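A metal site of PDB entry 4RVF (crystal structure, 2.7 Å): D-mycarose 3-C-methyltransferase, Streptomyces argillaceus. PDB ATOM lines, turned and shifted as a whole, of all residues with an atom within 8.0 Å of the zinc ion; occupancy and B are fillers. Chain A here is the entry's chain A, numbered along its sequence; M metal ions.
The zinc ion is bound by SG of Cys 13 (2.3 Å), SG of Cys 59 (2.3 Å), SG of Cys 56 (2.3 Å) and SG of Cys 16 (2.3 Å).
The zinc ion has four donor atoms within binding distance.
The backbone carbonyl oxygen (O) of Ala 18 sits at hydrogen-bond distance from the backbone NH (N) of Cys 13, 2.9 Å away.
The backbone NH (N) of Cys 56 sits at hydrogen-bond distance from the backbone carbonyl oxygen (O) of Leu 61, 2.9 Å away.
The backbone carbonyl oxygen of Cys 16 is in hydrogen-bond range of the guanidinium group of Arg 241, at 3.3 Å.
The side-chain sulfur (SG) of Cys 13 sits close to the backbone NH (N) of Met 15.
OG of Ser 58 lies close to SG of Cys 16 (3.7 Å).
SG of Cys 16 lies close to N of Ala 18, 3.6 Å away.
The backbone NH (N) of Leu 61 lies close to the side-chain sulfur (SG) of Cys 59 (3.7 Å).
N of Ser 58 sits close to SG of Cys 56 (3.6 Å).
The nearest printed residue that does not touch the zinc ion is Met 15 (4.6 Å).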
ATOM      1  N   THR A  12      -6.139  24.856   1.417  1.00  0.00           N
ATOM      2  CA  THR A  12      -4.802  25.055   0.873  1.00  0.00           C
ATOM      3  C   THR A  12      -4.829  25.144  -0.655  1.00  0.00           C
ATOM      4  O   THR A  12      -5.756  24.661  -1.312  1.00  0.00           O
ATOM      5  CB  THR A  12      -3.837  23.932   1.333  1.00  0.00           C
ATOM      6  OG1 THR A  12      -2.480  24.372   1.189  1.00  0.00           O
ATOM      7  CG2 THR A  12      -4.055  22.630   0.556  1.00  0.00           C
ATOM      8  N   CYS A  13      -3.793  25.774  -1.216  1.00  0.00           N
ATOM      9  CA  CYS A  13      -3.699  26.007  -2.656  1.00  0.00           C
ATOM     10  C   CYS A  13      -3.264  24.755  -3.420  1.00  0.00           C
ATOM     11  O   CYS A  13      -2.274  24.118  -3.070  1.00  0.00           O
ATOM     12  CB  CYS A  13      -2.719  27.161  -2.929  1.00  0.00           C
ATOM     13  SG  CYS A  13      -2.340  27.438  -4.671  1.00  0.00           S
ATOM     14  N   ARG A  14      -4.020  24.420  -4.463  1.00  0.00           N
ATOM     15  CA  ARG A  14      -3.787  23.224  -5.285  1.00  0.00           C
ATOM     16  C   ARG A  14      -2.370  23.098  -5.840  1.00  0.00           C
ATOM     17  O   ARG A  14      -1.835  22.002  -5.948  1.00  0.00           O
ATOM     18  CB  ARG A  14      -4.742  23.218  -6.485  1.00  0.00           C
ATOM     19  CG  ARG A  14      -6.106  22.629  -6.196  1.00  0.00           C
ATOM     20  CD  ARG A  14      -6.931  22.588  -7.471  1.00  0.00           C
ATOM     21  NE  ARG A  14      -7.387  23.913  -7.848  1.00  0.00           N
ATOM     22  CZ  ARG A  14      -8.539  24.463  -7.459  1.00  0.00           C
ATOM     23  NH1 ARG A  14      -9.394  23.795  -6.686  1.00  0.00           N
ATOM     24  NH2 ARG A  14      -8.841  25.684  -7.852  1.00  0.00           N
ATOM     25  N   MET A  15      -1.801  24.233  -6.232  1.00  0.00           N
ATOM     26  CA  MET A  15      -0.534  24.255  -6.956  1.00  0.00           C
ATOM     27  C   MET A  15       0.681  24.278  -6.024  1.00  0.00           C
ATOM     28  O   MET A  15       1.506  23.355  -6.060  1.00  0.00           O
ATOM     29  CB  MET A  15      -0.486  25.457  -7.897  1.00  0.00           C
ATOM     30  CG  MET A  15      -1.589  25.449  -8.961  1.00  0.00           C
ATOM     31  SD  MET A  15      -1.231  24.386 -10.366  1.00  0.00           S
ATOM     32  CE  MET A  15      -2.858  24.255 -11.104  1.00  0.00           C
ATOM     33  N   CYS A  16       0.776  25.310  -5.194  1.00  0.00           N
ATOM     34  CA  CYS A  16       1.989  25.553  -4.396  1.00  0.00           C
ATOM     35  C   CYS A  16       1.889  25.162  -2.911  1.00  0.00           C
ATOM     36  O   CYS A  16       2.915  25.055  -2.237  1.00  0.00           O
ATOM     37  CB  CYS A  16       2.422  27.022  -4.527  1.00  0.00           C
ATOM     38  SG  CYS A  16       1.445  28.179  -3.555  1.00  0.00           S
ATOM     39  N   GLY A  17       0.667  24.971  -2.414  1.00  0.00           N
ATOM     40  CA  GLY A  17       0.455  24.498  -1.036  1.00  0.00           C
ATOM     41  C   GLY A  17       0.278  25.584   0.009  1.00  0.00           C
ATOM     42  O   GLY A  17       0.028  25.286   1.177  1.00  0.00           O
ATOM     43  N   ALA A  18       0.412  26.843  -0.399  1.00  0.00           N
ATOM     44  CA  ALA A  18       0.248  27.982   0.504  1.00  0.00           C
ATOM     45  C   ALA A  18      -1.222  28.190   0.859  1.00  0.00           C
ATOM     46  O   ALA A  18      -2.108  27.522   0.322  1.00  0.00           O
ATOM     47  CB  ALA A  18       0.819  29.235  -0.128  1.00  0.00           C
ATOM     48  N   GLN A  19      -1.456  29.111   1.789  1.00  0.00           N
ATOM     49  CA  GLN A  19      -2.810  29.511   2.182  1.00  0.00           C
ATOM     50  C   GLN A  19      -2.813  31.004   2.476  1.00  0.00           C
ATOM     51  O   GLN A  19      -2.832  31.422   3.639  1.00  0.00           O
ATOM     52  CB  GLN A  19      -3.313  28.701   3.376  1.00  0.00           C
ATOM     53  CG  GLN A  19      -4.726  29.068   3.801  1.00  0.00           C
ATOM     54  CD  GLN A  19      -5.434  27.958   4.563  1.00  0.00           C
ATOM     55  OE1 GLN A  19      -4.792  27.108   5.199  1.00  0.00           O
ATOM     56  NE2 GLN A  19      -6.764  27.951   4.504  1.00  0.00           N
ATOM     57  N   ASP A  20      -2.775  31.795   1.410  1.00  0.00           N
ATOM     58  CA  ASP A  20      -2.746  33.258   1.499  1.00  0.00           C
ATOM     59  C   ASP A  20      -3.574  33.813   0.340  1.00  0.00           C
ATOM     60  O   ASP A  20      -3.044  34.178  -0.706  1.00  0.00           O
ATOM     61  CB  ASP A  20      -1.307  33.765   1.456  1.00  0.00           C
ATOM     62  CG  ASP A  20      -1.196  35.268   1.661  1.00  0.00           C
ATOM     63  OD1 ASP A  20      -0.093  35.815   1.436  1.00  0.00           O
ATOM     64  OD2 ASP A  20      -2.198  35.917   2.039  1.00  0.00           O
ATOM     65  N   TRP A  21      -4.886  33.874   0.557  1.00  0.00           N
ATOM     66  CA  TRP A  21      -5.846  34.186  -0.508  1.00  0.00           C
ATOM     67  C   TRP A  21      -6.296  35.646  -0.499  1.00  0.00           C
ATOM     68  O   TRP A  21      -6.800  36.154   0.502  1.00  0.00           O
ATOM     69  CB  TRP A  21      -7.087  33.305  -0.364  1.00  0.00           C
ATOM     70  CG  TRP A  21      -6.834  31.828  -0.498  1.00  0.00           C
ATOM     71  CD1 TRP A  21      -6.936  30.898   0.496  1.00  0.00           C
ATOM     72  CD2 TRP A  21      -6.479  31.117  -1.681  1.00  0.00           C
ATOM     73  NE1 TRP A  21      -6.645  29.649   0.010  1.00  0.00           N
ATOM     74  CE2 TRP A  21      -6.362  29.756  -1.332  1.00  0.00           C
ATOM     75  CE3 TRP A  21      -6.225  31.492  -3.003  1.00  0.00           C
ATOM     76  CZ2 TRP A  21      -6.011  28.770  -2.254  1.00  0.00           C
ATOM     77  CZ3 TRP A  21      -5.887  30.505  -3.932  1.00  0.00           C
ATOM     78  CH2 TRP A  21      -5.776  29.161  -3.543  1.00  0.00           C
ATOM     79  N   SER A  55      -7.194  34.745  -5.326  1.00  0.00           N
ATOM     80  CA  SER A  55      -5.851  34.667  -5.907  1.00  0.00           C
ATOM     81  C   SER A  55      -4.810  34.329  -4.845  1.00  0.00           C
ATOM     82  O   SER A  55      -4.715  34.986  -3.805  1.00  0.00           O
ATOM     83  CB  SER A  55      -5.483  35.991  -6.582  1.00  0.00           C
ATOM     84  OG  SER A  55      -4.280  35.854  -7.319  1.00  0.00           O
ATOM     85  N   CYS A  56      -4.032  33.286  -5.118  1.00  0.00           N
ATOM     86  CA  CYS A  56      -2.977  32.834  -4.213  1.00  0.00           C
ATOM     87  C   CYS A  56      -1.789  33.799  -4.260  1.00  0.00           C
ATOM     88  O   CYS A  56      -1.088  33.870  -5.261  1.00  0.00           O
ATOM     89  CB  CYS A  56      -2.522  31.426  -4.612  1.00  0.00           C
ATOM     90  SG  CYS A  56      -0.966  30.892  -3.898  1.00  0.00           S
ATOM     91  N   ARG A  57      -1.565  34.531  -3.176  1.00  0.00           N
ATOM     92  CA  ARG A  57      -0.487  35.542  -3.141  1.00  0.00           C
ATOM     93  C   ARG A  57       0.914  34.957  -3.350  1.00  0.00           C
ATOM     94  O   ARG A  57       1.802  35.649  -3.834  1.00  0.00           O
ATOM     95  CB  ARG A  57      -0.537  36.337  -1.839  1.00  0.00           C
ATOM     96  CG  ARG A  57      -1.706  37.313  -1.749  1.00  0.00           C
ATOM     97  CD  ARG A  57      -1.467  38.398  -0.712  1.00  0.00           C
ATOM     98  NE  ARG A  57      -2.464  39.462  -0.775  1.00  0.00           N
ATOM     99  CZ  ARG A  57      -3.645  39.460  -0.150  1.00  0.00           C
ATOM    100  NH1 ARG A  57      -4.014  38.439   0.612  1.00  0.00           N
ATOM    101  NH2 ARG A  57      -4.462  40.500  -0.291  1.00  0.00           N
ATOM    102  N   SER A  58       1.103  33.692  -2.987  1.00  0.00           N
ATOM    103  CA  SER A  58       2.374  32.988  -3.209  1.00  0.00           C
ATOM    104  C   SER A  58       2.685  32.728  -4.687  1.00  0.00           C
ATOM    105  O   SER A  58       3.641  33.282  -5.232  1.00  0.00           O
ATOM    106  CB  SER A  58       2.393  31.673  -2.431  1.00  0.00           C
ATOM    107  OG  SER A  58       3.618  30.989  -2.643  1.00  0.00           O
ATOM    108  N   CYS A  59       1.887  31.880  -5.338  1.00  0.00           N
ATOM    109  CA  CYS A  59       2.135  31.469  -6.728  1.00  0.00           C
ATOM    110  C   CYS A  59       1.188  32.106  -7.759  1.00  0.00           C
ATOM    111  O   CYS A  59       1.395  31.965  -8.961  1.00  0.00           O
ATOM    112  CB  CYS A  59       2.077  29.942  -6.837  1.00  0.00           C
ATOM    113  SG  CYS A  59       0.417  29.241  -6.917  1.00  0.00           S
ATOM    114  N   ARG A  60       0.151  32.785  -7.273  1.00  0.00           N
ATOM    115  CA  ARG A  60      -0.827  33.517  -8.103  1.00  0.00           C
ATOM    116  C   ARG A  60      -1.671  32.653  -9.038  1.00  0.00           C
ATOM    117  O   ARG A  60      -2.050  33.080 -10.133  1.00  0.00           O
ATOM    118  CB  ARG A  60      -0.165  34.696  -8.841  1.00  0.00           C
ATOM    119  CG  ARG A  60       0.184  35.855  -7.919  1.00  0.00           C
ATOM    120  CD  ARG A  60      -1.042  36.518  -7.309  1.00  0.00           C
ATOM    121  NE  ARG A  60      -0.689  37.683  -6.495  1.00  0.00           N
ATOM    122  CZ  ARG A  60      -1.570  38.463  -5.869  1.00  0.00           C
ATOM    123  NH1 ARG A  60      -2.875  38.233  -5.956  1.00  0.00           N
ATOM    124  NH2 ARG A  60      -1.130  39.497  -5.155  1.00  0.00           N
ATOM    125  N   LEU A  61      -2.001  31.446  -8.582  1.00  0.00           N
ATOM    126  CA  LEU A  61      -3.111  30.712  -9.151  1.00  0.00           C
ATOM    127  C   LEU A  61      -4.369  31.452  -8.748  1.00  0.00           C
ATOM    128  O   LEU A  61      -4.488  31.902  -7.608  1.00  0.00           O
ATOM    129  CB  LEU A  61      -3.180  29.284  -8.594  1.00  0.00           C
ATOM    130  CG  LEU A  61      -4.506  28.552  -8.828  1.00  0.00           C
ATOM    131  CD1 LEU A  61      -4.683  28.212 -10.296  1.00  0.00           C
ATOM    132  CD2 LEU A  61      -4.635  27.298  -7.972  1.00  0.00           C
ATOM    133  N   MET A  62      -5.308  31.583  -9.685  1.00  0.00           N
ATOM    134  CA  MET A  62      -6.649  32.038  -9.347  1.00  0.00           C
ATOM    135  C   MET A  62      -7.529  30.801  -9.240  1.00  0.00           C
ATOM    136  O   MET A  62      -7.498  29.926 -10.111  1.00  0.00           O
ATOM    137  CB  MET A  62      -7.186  33.028 -10.382  1.00  0.00           C
ATOM    138  CG  MET A  62      -8.342  33.880  -9.873  1.00  0.00           C
ATOM    139  SD  MET A  62      -8.666  35.353 -10.875  1.00  0.00           S
ATOM    140  CE  MET A  62      -9.411  34.616 -12.331  1.00  0.00           C
ATOM    141  N   SER A 234       2.450  29.590 -11.857  1.00  0.00           N
ATOM    142  CA  SER A 234       1.793  28.662 -10.939  1.00  0.00           C
ATOM    143  C   SER A 234       2.048  27.194 -11.311  1.00  0.00           C
ATOM    144  O   SER A 234       2.120  26.339 -10.431  1.00  0.00           O
ATOM    145  CB  SER A 234       0.291  28.923 -10.908  1.00  0.00           C
ATOM    146  OG  SER A 234      -0.276  28.756 -12.197  1.00  0.00           O
ATOM    147  N   ALA A 237       5.577  26.332 -10.324  1.00  0.00           N
ATOM    148  CA  ALA A 237       5.549  26.141  -8.873  1.00  0.00           C
ATOM    149  C   ALA A 237       5.108  24.727  -8.504  1.00  0.00           C
ATOM    150  O   ALA A 237       5.705  24.080  -7.643  1.00  0.00           O
ATOM    151  CB  ALA A 237       4.650  27.165  -8.215  1.00  0.00           C
ATOM    152  N   LEU A 238       4.049  24.259  -9.157  1.00  0.00           N
ATOM    153  CA  LEU A 238       3.533  22.902  -8.933  1.00  0.00           C
ATOM    154  C   LEU A 238       4.539  21.838  -9.386  1.00  0.00           C
ATOM    155  O   LEU A 238       4.893  20.950  -8.621  1.00  0.00           O
ATOM    156  CB  LEU A 238       2.220  22.703  -9.696  1.00  0.00           C
ATOM    157  CG  LEU A 238       1.679  21.262  -9.706  1.00  0.00           C
ATOM    158  CD1 LEU A 238       0.849  20.969  -8.452  1.00  0.00           C
ATOM    159  CD2 LEU A 238       0.873  21.016 -10.969  1.00  0.00           C
ATOM    160  N   ARG A 241       7.614  20.737  -7.420  1.00  0.00           N
ATOM    161  CA  ARG A 241       7.399  19.873  -6.250  1.00  0.00           C
ATOM    162  C   ARG A 241       7.231  18.389  -6.572  1.00  0.00           C
ATOM    163  O   ARG A 241       7.142  17.567  -5.661  1.00  0.00           O
ATOM    164  CB  ARG A 241       6.173  20.349  -5.474  1.00  0.00           C
ATOM    165  CG  ARG A 241       6.187  21.824  -5.092  1.00  0.00           C
ATOM    166  CD  ARG A 241       5.149  22.127  -4.025  1.00  0.00           C
ATOM    167  NE  ARG A 241       3.807  21.709  -4.426  1.00  0.00           N
ATOM    168  CZ  ARG A 241       2.766  21.555  -3.597  1.00  0.00           C
ATOM    169  NH1 ARG A 241       2.903  21.782  -2.290  1.00  0.00           N
ATOM    170  NH2 ARG A 241       1.596  21.178  -4.077  1.00  0.00           N
HETATM  171 ZN    ZN M   1      -0.451  28.798  -4.797  1.00  0.00          ZN
